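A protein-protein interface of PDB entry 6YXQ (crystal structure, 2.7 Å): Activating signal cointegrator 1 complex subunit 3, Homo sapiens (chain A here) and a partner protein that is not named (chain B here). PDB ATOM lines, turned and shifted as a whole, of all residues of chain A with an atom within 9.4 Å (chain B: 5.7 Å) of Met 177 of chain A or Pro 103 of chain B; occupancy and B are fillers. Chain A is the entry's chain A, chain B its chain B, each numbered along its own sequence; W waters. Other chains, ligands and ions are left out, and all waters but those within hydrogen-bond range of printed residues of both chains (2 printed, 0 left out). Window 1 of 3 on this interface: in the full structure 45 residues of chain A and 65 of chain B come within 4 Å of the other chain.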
ATOM      1  N   GLU A   3     -26.483  11.500  -2.657  1.00  0.00           N
ATOM      2  CA  GLU A   3     -25.498  12.522  -2.993  1.00  0.00           C
ATOM      3  C   GLU A   3     -25.736  13.762  -2.153  1.00  0.00           C
ATOM      4  O   GLU A   3     -26.808  14.363  -2.214  1.00  0.00           O
ATOM      5  CB  GLU A   3     -25.557  12.880  -4.479  1.00  0.00           C
ATOM      6  CG  GLU A   3     -24.643  14.037  -4.859  1.00  0.00           C
ATOM      7  CD  GLU A   3     -24.954  14.609  -6.226  1.00  0.00           C
ATOM      8  OE1 GLU A   3     -26.001  14.240  -6.800  1.00  0.00           O
ATOM      9  OE2 GLU A   3     -24.153  15.428  -6.727  1.00  0.00           O
ATOM     10  N   PHE A   4     -24.725  14.146  -1.371  1.00  0.00           N
ATOM     11  CA  PHE A   4     -24.898  15.254  -0.439  1.00  0.00           C
ATOM     12  C   PHE A   4     -24.554  16.588  -1.084  1.00  0.00           C
ATOM     13  O   PHE A   4     -25.065  17.631  -0.657  1.00  0.00           O
ATOM     14  CB  PHE A   4     -24.087  15.002   0.840  1.00  0.00           C
ATOM     15  CG  PHE A   4     -24.542  13.780   1.628  1.00  0.00           C
ATOM     16  CD1 PHE A   4     -24.012  13.499   2.880  1.00  0.00           C
ATOM     17  CD2 PHE A   4     -25.500  12.914   1.109  1.00  0.00           C
ATOM     18  CE1 PHE A   4     -24.433  12.377   3.594  1.00  0.00           C
ATOM     19  CE2 PHE A   4     -25.919  11.799   1.809  1.00  0.00           C
ATOM     20  CZ  PHE A   4     -25.384  11.526   3.055  1.00  0.00           C
ATOM     21  N   MET A   5     -23.721  16.570  -2.125  1.00  0.00           N
ATOM     22  CA  MET A   5     -23.594  17.721  -3.010  1.00  0.00           C
ATOM     23  C   MET A   5     -24.918  18.070  -3.681  1.00  0.00           C
ATOM     24  O   MET A   5     -25.061  19.175  -4.217  1.00  0.00           O
ATOM     25  CB  MET A   5     -22.527  17.448  -4.078  1.00  0.00           C
ATOM     26  CG  MET A   5     -21.215  16.882  -3.545  1.00  0.00           C
ATOM     27  SD  MET A   5     -19.769  17.510  -4.433  1.00  0.00           S
ATOM     28  CE  MET A   5     -20.369  17.512  -6.125  1.00  0.00           C
ATOM     29  N   LEU A   7     -27.947  17.932  -1.996  1.00  0.00           N
ATOM     30  CA  LEU A   7     -28.983  18.309  -1.042  1.00  0.00           C
ATOM     31  C   LEU A   7     -29.276  19.805  -1.121  1.00  0.00           C
ATOM     32  O   LEU A   7     -28.350  20.623  -1.181  1.00  0.00           O
ATOM     33  CB  LEU A   7     -28.601  17.958   0.395  1.00  0.00           C
ATOM     34  CG  LEU A   7     -28.254  16.550   0.861  1.00  0.00           C
ATOM     35  CD1 LEU A   7     -27.133  16.692   1.853  1.00  0.00           C
ATOM     36  CD2 LEU A   7     -29.460  15.846   1.488  1.00  0.00           C
ATOM     37  N   ARG A   9     -29.777  23.422  -0.203  1.00  0.00           N
ATOM     38  CA  ARG A   9     -29.358  24.261   0.910  1.00  0.00           C
ATOM     39  C   ARG A   9     -29.515  25.734   0.561  1.00  0.00           C
ATOM     40  O   ARG A   9     -29.241  26.160  -0.568  1.00  0.00           O
ATOM     41  CB  ARG A   9     -27.905  23.968   1.317  1.00  0.00           C
ATOM     42  CG  ARG A   9     -27.671  22.518   1.724  1.00  0.00           C
ATOM     43  CD  ARG A   9     -26.469  22.366   2.638  1.00  0.00           C
ATOM     44  NE  ARG A   9     -26.502  21.107   3.373  1.00  0.00           N
ATOM     45  CZ  ARG A   9     -25.710  20.070   3.122  1.00  0.00           C
ATOM     46  NH1 ARG A   9     -25.813  18.965   3.848  1.00  0.00           N
ATOM     47  NH2 ARG A   9     -24.815  20.137   2.146  1.00  0.00           N
ATOM     48  N   PHE A 173     -13.813  24.295  22.729  1.00  0.00           N
ATOM     49  CA  PHE A 173     -14.516  24.063  21.477  1.00  0.00           C
ATOM     50  C   PHE A 173     -15.528  22.951  21.674  1.00  0.00           C
ATOM     51  O   PHE A 173     -15.275  21.991  22.404  1.00  0.00           O
ATOM     52  CB  PHE A 173     -13.545  23.694  20.351  1.00  0.00           C
ATOM     53  CG  PHE A 173     -14.213  23.425  19.033  1.00  0.00           C
ATOM     54  CD1 PHE A 173     -14.760  24.460  18.294  1.00  0.00           C
ATOM     55  CD2 PHE A 173     -14.283  22.142  18.527  1.00  0.00           C
ATOM     56  CE1 PHE A 173     -15.373  24.214  17.081  1.00  0.00           C
ATOM     57  CE2 PHE A 173     -14.892  21.891  17.310  1.00  0.00           C
ATOM     58  CZ  PHE A 173     -15.439  22.928  16.589  1.00  0.00           C
ATOM     59  N   SER A 174     -16.671  23.086  21.014  1.00  0.00           N
ATOM     60  CA  SER A 174     -17.764  22.140  21.141  1.00  0.00           C
ATOM     61  C   SER A 174     -18.082  21.552  19.780  1.00  0.00           C
ATOM     62  O   SER A 174     -18.073  22.260  18.768  1.00  0.00           O
ATOM     63  CB  SER A 174     -19.009  22.807  21.729  1.00  0.00           C
ATOM     64  OG  SER A 174     -20.088  21.892  21.809  1.00  0.00           O
ATOM     65  N   PHE A 175     -18.349  20.250  19.759  1.00  0.00           N
ATOM     66  CA  PHE A 175     -18.767  19.561  18.550  1.00  0.00           C
ATOM     67  C   PHE A 175     -20.277  19.410  18.477  1.00  0.00           C
ATOM     68  O   PHE A 175     -20.780  18.687  17.612  1.00  0.00           O
ATOM     69  CB  PHE A 175     -18.089  18.193  18.459  1.00  0.00           C
ATOM     70  CG  PHE A 175     -16.613  18.269  18.204  1.00  0.00           C
ATOM     71  CD1 PHE A 175     -15.731  18.551  19.233  1.00  0.00           C
ATOM     72  CD2 PHE A 175     -16.106  18.069  16.931  1.00  0.00           C
ATOM     73  CE1 PHE A 175     -14.372  18.626  18.997  1.00  0.00           C
ATOM     74  CE2 PHE A 175     -14.746  18.144  16.688  1.00  0.00           C
ATOM     75  CZ  PHE A 175     -13.879  18.423  17.722  1.00  0.00           C
ATOM     76  N   ASP A 176     -21.007  20.069  19.374  1.00  0.00           N
ATOM     77  CA  ASP A 176     -22.462  20.044  19.340  1.00  0.00           C
ATOM     78  C   ASP A 176     -22.965  20.892  18.177  1.00  0.00           C
ATOM     79  O   ASP A 176     -22.665  22.089  18.095  1.00  0.00           O
ATOM     80  CB  ASP A 176     -23.019  20.556  20.664  1.00  0.00           C
ATOM     81  CG  ASP A 176     -24.282  19.840  21.079  1.00  0.00           C
ATOM     82  OD1 ASP A 176     -24.769  18.997  20.293  1.00  0.00           O
ATOM     83  OD2 ASP A 176     -24.791  20.124  22.185  1.00  0.00           O
ATOM     84  N   MET A 177     -23.723  20.278  17.274  1.00  0.00           N
ATOM     85  CA  MET A 177     -24.248  20.956  16.098  1.00  0.00           C
ATOM     86  C   MET A 177     -25.766  21.020  16.171  1.00  0.00           C
ATOM     87  O   MET A 177     -26.405  20.183  16.813  1.00  0.00           O
ATOM     88  CB  MET A 177     -23.816  20.247  14.809  1.00  0.00           C
ATOM     89  CG  MET A 177     -22.321  20.256  14.584  1.00  0.00           C
ATOM     90  SD  MET A 177     -21.834  19.243  13.180  1.00  0.00           S
ATOM     91  CE  MET A 177     -22.444  20.232  11.820  1.00  0.00           C
ATOM     92  N   HIS A 178     -26.339  22.023  15.506  1.00  0.00           N
ATOM     93  CA  HIS A 178     -27.788  22.181  15.505  1.00  0.00           C
ATOM     94  C   HIS A 178     -28.451  20.958  14.886  1.00  0.00           C
ATOM     95  O   HIS A 178     -28.082  20.523  13.790  1.00  0.00           O
ATOM     96  CB  HIS A 178     -28.186  23.444  14.741  1.00  0.00           C
ATOM     97  CG  HIS A 178     -28.042  24.703  15.536  1.00  0.00           C
ATOM     98  ND1 HIS A 178     -28.561  24.848  16.805  1.00  0.00           N
ATOM     99  CD2 HIS A 178     -27.437  25.878  15.243  1.00  0.00           C
ATOM    100  CE1 HIS A 178     -28.281  26.056  17.259  1.00  0.00           C
ATOM    101  NE2 HIS A 178     -27.599  26.702  16.330  1.00  0.00           N
ATOM    102  N   ASP A 179     -29.430  20.402  15.597  1.00  0.00           N
ATOM    103  CA  ASP A 179     -30.147  19.203  15.181  1.00  0.00           C
ATOM    104  C   ASP A 179     -31.628  19.520  15.002  1.00  0.00           C
ATOM    105  O   ASP A 179     -32.076  20.655  15.194  1.00  0.00           O
ATOM    106  CB  ASP A 179     -29.955  18.075  16.200  1.00  0.00           C
ATOM    107  CG  ASP A 179     -29.893  16.705  15.552  1.00  0.00           C
ATOM    108  OD1 ASP A 179     -30.109  16.609  14.328  1.00  0.00           O
ATOM    109  OD2 ASP A 179     -29.623  15.719  16.269  1.00  0.00           O
ATOM    110  N   LEU A 180     -32.387  18.496  14.621  1.00  0.00           N
ATOM    111  CA  LEU A 180     -33.834  18.619  14.558  1.00  0.00           C
ATOM    112  C   LEU A 180     -34.392  18.597  15.970  1.00  0.00           C
ATOM    113  O   LEU A 180     -34.004  17.755  16.786  1.00  0.00           O
ATOM    114  CB  LEU A 180     -34.445  17.488  13.731  1.00  0.00           C
ATOM    115  CG  LEU A 180     -34.186  17.462  12.229  1.00  0.00           C
ATOM    116  CD1 LEU A 180     -34.539  16.092  11.673  1.00  0.00           C
ATOM    117  CD2 LEU A 180     -34.979  18.546  11.534  1.00  0.00           C
ATOM    118  N   ASP A 181     -35.283  19.535  16.264  1.00  0.00           N
ATOM    119  CA  ASP A 181     -36.006  19.479  17.521  1.00  0.00           C
ATOM    120  C   ASP A 181     -36.963  18.298  17.507  1.00  0.00           C
ATOM    121  O   ASP A 181     -37.516  17.920  16.469  1.00  0.00           O
ATOM    122  CB  ASP A 181     -36.761  20.780  17.776  1.00  0.00           C
ATOM    123  CG  ASP A 181     -35.875  21.849  18.382  1.00  0.00           C
ATOM    124  OD1 ASP A 181     -34.703  21.552  18.686  1.00  0.00           O
ATOM    125  OD2 ASP A 181     -36.345  22.988  18.554  1.00  0.00           O
ATOM    126  N   TYR B  44     -13.050  20.356  -0.932  1.00  0.00           N
ATOM    127  CA  TYR B  44     -13.630  19.381  -0.022  1.00  0.00           C
ATOM    128  C   TYR B  44     -14.863  18.751  -0.662  1.00  0.00           C
ATOM    129  O   TYR B  44     -15.707  19.456  -1.227  1.00  0.00           O
ATOM    130  CB  TYR B  44     -13.991  20.047   1.309  1.00  0.00           C
ATOM    131  CG  TYR B  44     -14.786  19.176   2.257  1.00  0.00           C
ATOM    132  CD1 TYR B  44     -16.173  19.119   2.189  1.00  0.00           C
ATOM    133  CD2 TYR B  44     -14.148  18.417   3.231  1.00  0.00           C
ATOM    134  CE1 TYR B  44     -16.901  18.325   3.051  1.00  0.00           C
ATOM    135  CE2 TYR B  44     -14.873  17.622   4.099  1.00  0.00           C
ATOM    136  CZ  TYR B  44     -16.247  17.580   4.004  1.00  0.00           C
ATOM    137  OH  TYR B  44     -16.968  16.793   4.866  1.00  0.00           O
ATOM    138  N   PRO B  46     -17.939  15.837   0.466  1.00  0.00           N
ATOM    139  CA  PRO B  46     -18.459  15.123   1.639  1.00  0.00           C
ATOM    140  C   PRO B  46     -18.406  13.619   1.438  1.00  0.00           C
ATOM    141  O   PRO B  46     -18.261  13.140   0.302  1.00  0.00           O
ATOM    142  CB  PRO B  46     -19.906  15.625   1.737  1.00  0.00           C
ATOM    143  CG  PRO B  46     -20.261  15.986   0.332  1.00  0.00           C
ATOM    144  CD  PRO B  46     -19.003  16.518  -0.290  1.00  0.00           C
ATOM    145  N   PRO B  47     -18.520  12.842   2.514  1.00  0.00           N
ATOM    146  CA  PRO B  47     -18.396  11.372   2.413  1.00  0.00           C
ATOM    147  C   PRO B  47     -19.548  10.755   1.638  1.00  0.00           C
ATOM    148  O   PRO B  47     -20.608  11.378   1.485  1.00  0.00           O
ATOM    149  CB  PRO B  47     -18.410  10.919   3.884  1.00  0.00           C
ATOM    150  CG  PRO B  47     -18.971  12.063   4.651  1.00  0.00           C
ATOM    151  CD  PRO B  47     -18.554  13.294   3.917  1.00  0.00           C
ATOM    152  N   TYR B 101     -20.596  22.268   1.563  1.00  0.00           N
ATOM    153  CA  TYR B 101     -20.964  20.872   1.356  1.00  0.00           C
ATOM    154  C   TYR B 101     -20.918  19.993   2.599  1.00  0.00           C
ATOM    155  O   TYR B 101     -21.445  18.876   2.549  1.00  0.00           O
ATOM    156  CB  TYR B 101     -20.077  20.255   0.265  1.00  0.00           C
ATOM    157  CG  TYR B 101     -20.353  20.821  -1.112  1.00  0.00           C
ATOM    158  CD1 TYR B 101     -21.588  20.641  -1.727  1.00  0.00           C
ATOM    159  CD2 TYR B 101     -19.383  21.536  -1.796  1.00  0.00           C
ATOM    160  CE1 TYR B 101     -21.848  21.163  -2.988  1.00  0.00           C
ATOM    161  CE2 TYR B 101     -19.633  22.059  -3.057  1.00  0.00           C
ATOM    162  CZ  TYR B 101     -20.864  21.871  -3.647  1.00  0.00           C
ATOM    163  OH  TYR B 101     -21.098  22.393  -4.899  1.00  0.00           O
ATOM    164  N   VAL B 102     -20.342  20.453   3.708  1.00  0.00           N
ATOM    165  CA  VAL B 102     -20.204  19.578   4.877  1.00  0.00           C
ATOM    166  C   VAL B 102     -21.588  19.196   5.384  1.00  0.00           C
ATOM    167  O   VAL B 102     -22.483  20.059   5.459  1.00  0.00           O
ATOM    168  CB  VAL B 102     -19.374  20.266   5.977  1.00  0.00           C
ATOM    169  CG1 VAL B 102     -20.000  21.579   6.407  1.00  0.00           C
ATOM    170  CG2 VAL B 102     -19.208  19.345   7.176  1.00  0.00           C
ATOM    171  N   PRO B 103     -21.837  17.929   5.701  1.00  0.00           N
ATOM    172  CA  PRO B 103     -23.171  17.541   6.171  1.00  0.00           C
ATOM    173  C   PRO B 103     -23.507  18.211   7.494  1.00  0.00           C
ATOM    174  O   PRO B 103     -22.684  18.269   8.412  1.00  0.00           O
ATOM    175  CB  PRO B 103     -23.071  16.016   6.312  1.00  0.00           C
ATOM    176  CG  PRO B 103     -21.607  15.735   6.418  1.00  0.00           C
ATOM    177  CD  PRO B 103     -20.944  16.768   5.557  1.00  0.00           C
ATOM    178  N   ARG B 104     -24.724  18.740   7.573  1.00  0.00           N
ATOM    179  CA  ARG B 104     -25.268  19.254   8.817  1.00  0.00           C
ATOM    180  C   ARG B 104     -25.840  18.104   9.637  1.00  0.00           C
ATOM    181  O   ARG B 104     -26.250  17.068   9.100  1.00  0.00           O
ATOM    182  CB  ARG B 104     -26.353  20.304   8.551  1.00  0.00           C
ATOM    183  CG  ARG B 104     -25.835  21.645   8.042  1.00  0.00           C
ATOM    184  CD  ARG B 104     -25.626  21.625   6.537  1.00  0.00           C
ATOM    185  NE  ARG B 104     -25.386  22.951   5.980  1.00  0.00           N
ATOM    186  CZ  ARG B 104     -24.238  23.339   5.430  1.00  0.00           C
ATOM    187  NH1 ARG B 104     -23.216  22.501   5.353  1.00  0.00           N
ATOM    188  NH2 ARG B 104     -24.115  24.566   4.949  1.00  0.00           N
ATOM    189  N   LYS B 105     -25.860  18.293  10.957  1.00  0.00           N
ATOM    190  CA  LYS B 105     -26.344  17.226  11.825  1.00  0.00           C
ATOM    191  C   LYS B 105     -27.797  16.890  11.526  1.00  0.00           C
ATOM    192  O   LYS B 105     -28.160  15.713  11.419  1.00  0.00           O
ATOM    193  CB  LYS B 105     -26.172  17.602  13.299  1.00  0.00           C
ATOM    194  CG  LYS B 105     -26.537  16.456  14.253  1.00  0.00           C
ATOM    195  CD  LYS B 105     -25.782  16.528  15.573  1.00  0.00           C
ATOM    196  CE  LYS B 105     -24.314  16.140  15.409  1.00  0.00           C
ATOM    197  NZ  LYS B 105     -23.562  16.156  16.702  1.00  0.00           N
ATOM    198  N   ASP B 107     -29.327  16.804   8.958  1.00  0.00           N
ATOM    199  CA  ASP B 107     -29.512  16.058   7.725  1.00  0.00           C
ATOM    200  C   ASP B 107     -29.701  14.571   8.016  1.00  0.00           C
ATOM    201  O   ASP B 107     -29.363  14.069   9.094  1.00  0.00           O
ATOM    202  CB  ASP B 107     -28.319  16.255   6.788  1.00  0.00           C
ATOM    203  CG  ASP B 107     -28.384  17.561   6.031  1.00  0.00           C
ATOM    204  OD1 ASP B 107     -29.506  17.993   5.681  1.00  0.00           O
ATOM    205  OD2 ASP B 107     -27.313  18.154   5.787  1.00  0.00           O
ATOM    206  N   GLN B 120     -13.765  13.772  10.125  1.00  0.00           N
ATOM    207  CA  GLN B 120     -14.746  14.848  10.057  1.00  0.00           C
ATOM    208  C   GLN B 120     -14.642  15.767  11.268  1.00  0.00           C
ATOM    209  O   GLN B 120     -14.746  16.993  11.137  1.00  0.00           O
ATOM    210  CB  GLN B 120     -16.148  14.260   9.944  1.00  0.00           C
ATOM    211  CG  GLN B 120     -16.499  13.808   8.544  1.00  0.00           C
ATOM    212  CD  GLN B 120     -17.226  14.869   7.763  1.00  0.00           C
ATOM    213  OE1 GLN B 120     -16.616  15.651   7.029  1.00  0.00           O
ATOM    214  NE2 GLN B 120     -18.547  14.909   7.918  1.00  0.00           N
ATOM    215  N   HIS B 124     -13.838  19.743  11.242  1.00  0.00           N
ATOM    216  CA  HIS B 124     -14.748  20.673  11.903  1.00  0.00           C
ATOM    217  C   HIS B 124     -13.984  21.632  12.814  1.00  0.00           C
ATOM    218  O   HIS B 124     -14.095  22.864  12.687  1.00  0.00           O
ATOM    219  CB  HIS B 124     -15.786  19.862  12.680  1.00  0.00           C
ATOM    220  CG  HIS B 124     -16.932  20.664  13.220  1.00  0.00           C
ATOM    221  ND1 HIS B 124     -16.993  21.078  14.533  1.00  0.00           N
ATOM    222  CD2 HIS B 124     -18.077  21.091  12.638  1.00  0.00           C
ATOM    223  CE1 HIS B 124     -18.118  21.740  14.733  1.00  0.00           C
ATOM    224  NE2 HIS B 124     -18.795  21.760  13.599  1.00  0.00           N
ATOM    225  N   VAL B 170     -24.950  28.062  11.375  1.00  0.00           N
ATOM    226  CA  VAL B 170     -25.684  26.807  11.513  1.00  0.00           C
ATOM    227  C   VAL B 170     -24.733  25.666  11.847  1.00  0.00           C
ATOM    228  O   VAL B 170     -25.132  24.679  12.481  1.00  0.00           O
ATOM    229  CB  VAL B 170     -26.505  26.496  10.254  1.00  0.00           C
ATOM    230  CG1 VAL B 170     -25.609  26.248   9.064  1.00  0.00           C
ATOM    231  CG2 VAL B 170     -27.408  25.297  10.482  1.00  0.00           C
ATOM    232  N   LEU B 171     -23.458  25.788  11.467  1.00  0.00           N
ATOM    233  CA  LEU B 171     -22.517  24.700  11.702  1.00  0.00           C
ATOM    234  C   LEU B 171     -21.927  24.733  13.112  1.00  0.00           C
ATOM    235  O   LEU B 171     -21.776  23.678  13.737  1.00  0.00           O
ATOM    236  CB  LEU B 171     -21.396  24.741  10.663  1.00  0.00           C
ATOM    237  CG  LEU B 171     -21.760  24.272   9.247  1.00  0.00           C
ATOM    238  CD1 LEU B 171     -20.593  24.515   8.299  1.00  0.00           C
ATOM    239  CD2 LEU B 171     -22.207  22.816   9.190  1.00  0.00           C
ATOM    240  N   LYS B 174     -24.506  25.939  17.902  1.00  0.00           N
ATOM    241  CA  LYS B 174     -25.083  25.271  19.062  1.00  0.00           C
ATOM    242  C   LYS B 174     -24.077  25.198  20.204  1.00  0.00           C
ATOM    243  O   LYS B 174     -24.382  25.576  21.341  1.00  0.00           O
ATOM    244  CB  LYS B 174     -25.574  23.875  18.686  1.00  0.00           C
ATOM    245  CG  LYS B 174     -26.677  23.372  19.609  1.00  0.00           C
ATOM    246  CD  LYS B 174     -26.665  21.858  19.749  1.00  0.00           C
ATOM    247  CE  LYS B 174     -27.907  21.365  20.481  1.00  0.00           C
ATOM    248  NZ  LYS B 174     -29.146  21.579  19.674  1.00  0.00           N
ATOM    249  N   GLY B 175     -22.866  24.737  19.915  1.00  0.00           N
ATOM    250  CA  GLY B 175     -21.874  24.578  20.953  1.00  0.00           C
ATOM    251  C   GLY B 175     -21.072  25.829  21.248  1.00  0.00           C
ATOM    252  O   GLY B 175     -21.007  26.274  22.399  1.00  0.00           O
HETATM  253  O   HOH W   1     -23.873  24.211  15.520  1.00  0.00           O
HETATM  254  O   HOH W   2     -25.932  20.969  11.746  1.00  0.00           O
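N of Asp 176 of chain A is in hydrogen-bond range of OG of Ser 174 of chain A, at 3.2 Å.
O of Val 102 of chain B sits at hydrogen-bond distance from NH1 of Arg 104 of chain B (2.6 Å).
The side-chain carboxylate (OD2) of Asp 107 of chain B sits at hydrogen-bond distance from the backbone NH (N) of Arg 104 of chain B (3.2 Å).
Water W2 lies within hydrogen-bond range of N of Lys 105 of chain B (2.8 Å) and O of His 178 of chain A (3.0 Å).
Water W1 lies within hydrogen-bond range of the backbone carbonyl oxygen of Leu 171 of chain B (2.8 Å), the backbone NH of Lys 174 of chain B (3.0 Å), the backbone NH of His 178 of chain A (3.3 Å) and the backbone carbonyl oxygen of Val 170 of chain B (3.3 Å).
Of the 15 printed residues of chain B, 12 touch a printed residue of chain A.
Hydrophobic or aromatic side chains of chain B that line the printed part of chain A: Pro 46, Tyr 101, His 124 and Leu 171.
Among the printed residues, 23 pairs touch across the chains.
Among the printed residues, Asp or Glu carboxylates within 4 Å of a Lys or Arg side-chain nitrogen of the other chain: Arg 9 of chain A with Asp 107 of chain B.
Among the printed residues, pairs that only touch across the chains: Phe 4 of chain A with Pro 46 of chain B, Met 5 of chain A with Pro 46 of chain B, Met 5 of chain A with Tyr 101 of chain B, Arg 9 of chain A with Tyr 101 of chain B, Arg 9 of chain A with Val 102 of chain B, Arg 9 of chain A with Pro 103 of chain B, Phe 173 of chain A with His 124 of chain B, Ser 174 of chain A with Gly 175 of chain B, Phe 175 of chain A with Lys 105 of chain B, Phe 175 of chain A with His 124 of chain B, Asp 176 of chain A with Lys 174 of chain B, Met 177 of chain A with Pro 103 of chain B, Met 177 of chain A with Lys 105 of chain B, Met 177 of chain A with His 124 of chain B, Met 177 of chain A with Leu 171 of chain B, Met 177 of chain A with Lys 174 of chain B, His 178 of chain A with Lys 105 of chain B, His 178 of chain A with Val 170 of chain B, His 178 of chain A with Lys 174 of chain B and Asp 179 of chain A with Lys 105 of chain B.
The guanidinium group (NH1) of Arg 9 of chain A lies within salt-bridge range of the side-chain carboxylate (OD2) of Asp 107 of chain B (2.6 Å).
N of Gly 175 of chain B lies within hydrogen-bond range of O of Asp 176 of chain A, at 3.2 Å.
NE of Arg 104 of chain B lies close to NE of Arg 9 of chain A (3.4 Å).
Of chain A, only Arg 9 and Met 177 come within 4 Å of Pro 103 of chain B.
Of the printed residues of chain A, Gly 175 of chain B touches Ser 174 and Asp 176.
Printed residues of chain B within 4 Å of Phe 175 of chain A: Lys 105 and His 124.
Gln 120 of chain B touches none of the printed residues of chain A.
Glu 3 of chain A touches none of the printed residues of chain B.
The nearest residue of chain A that does not touch Pro 103 of chain B is Phe 4 of chain A (4.4 Å).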
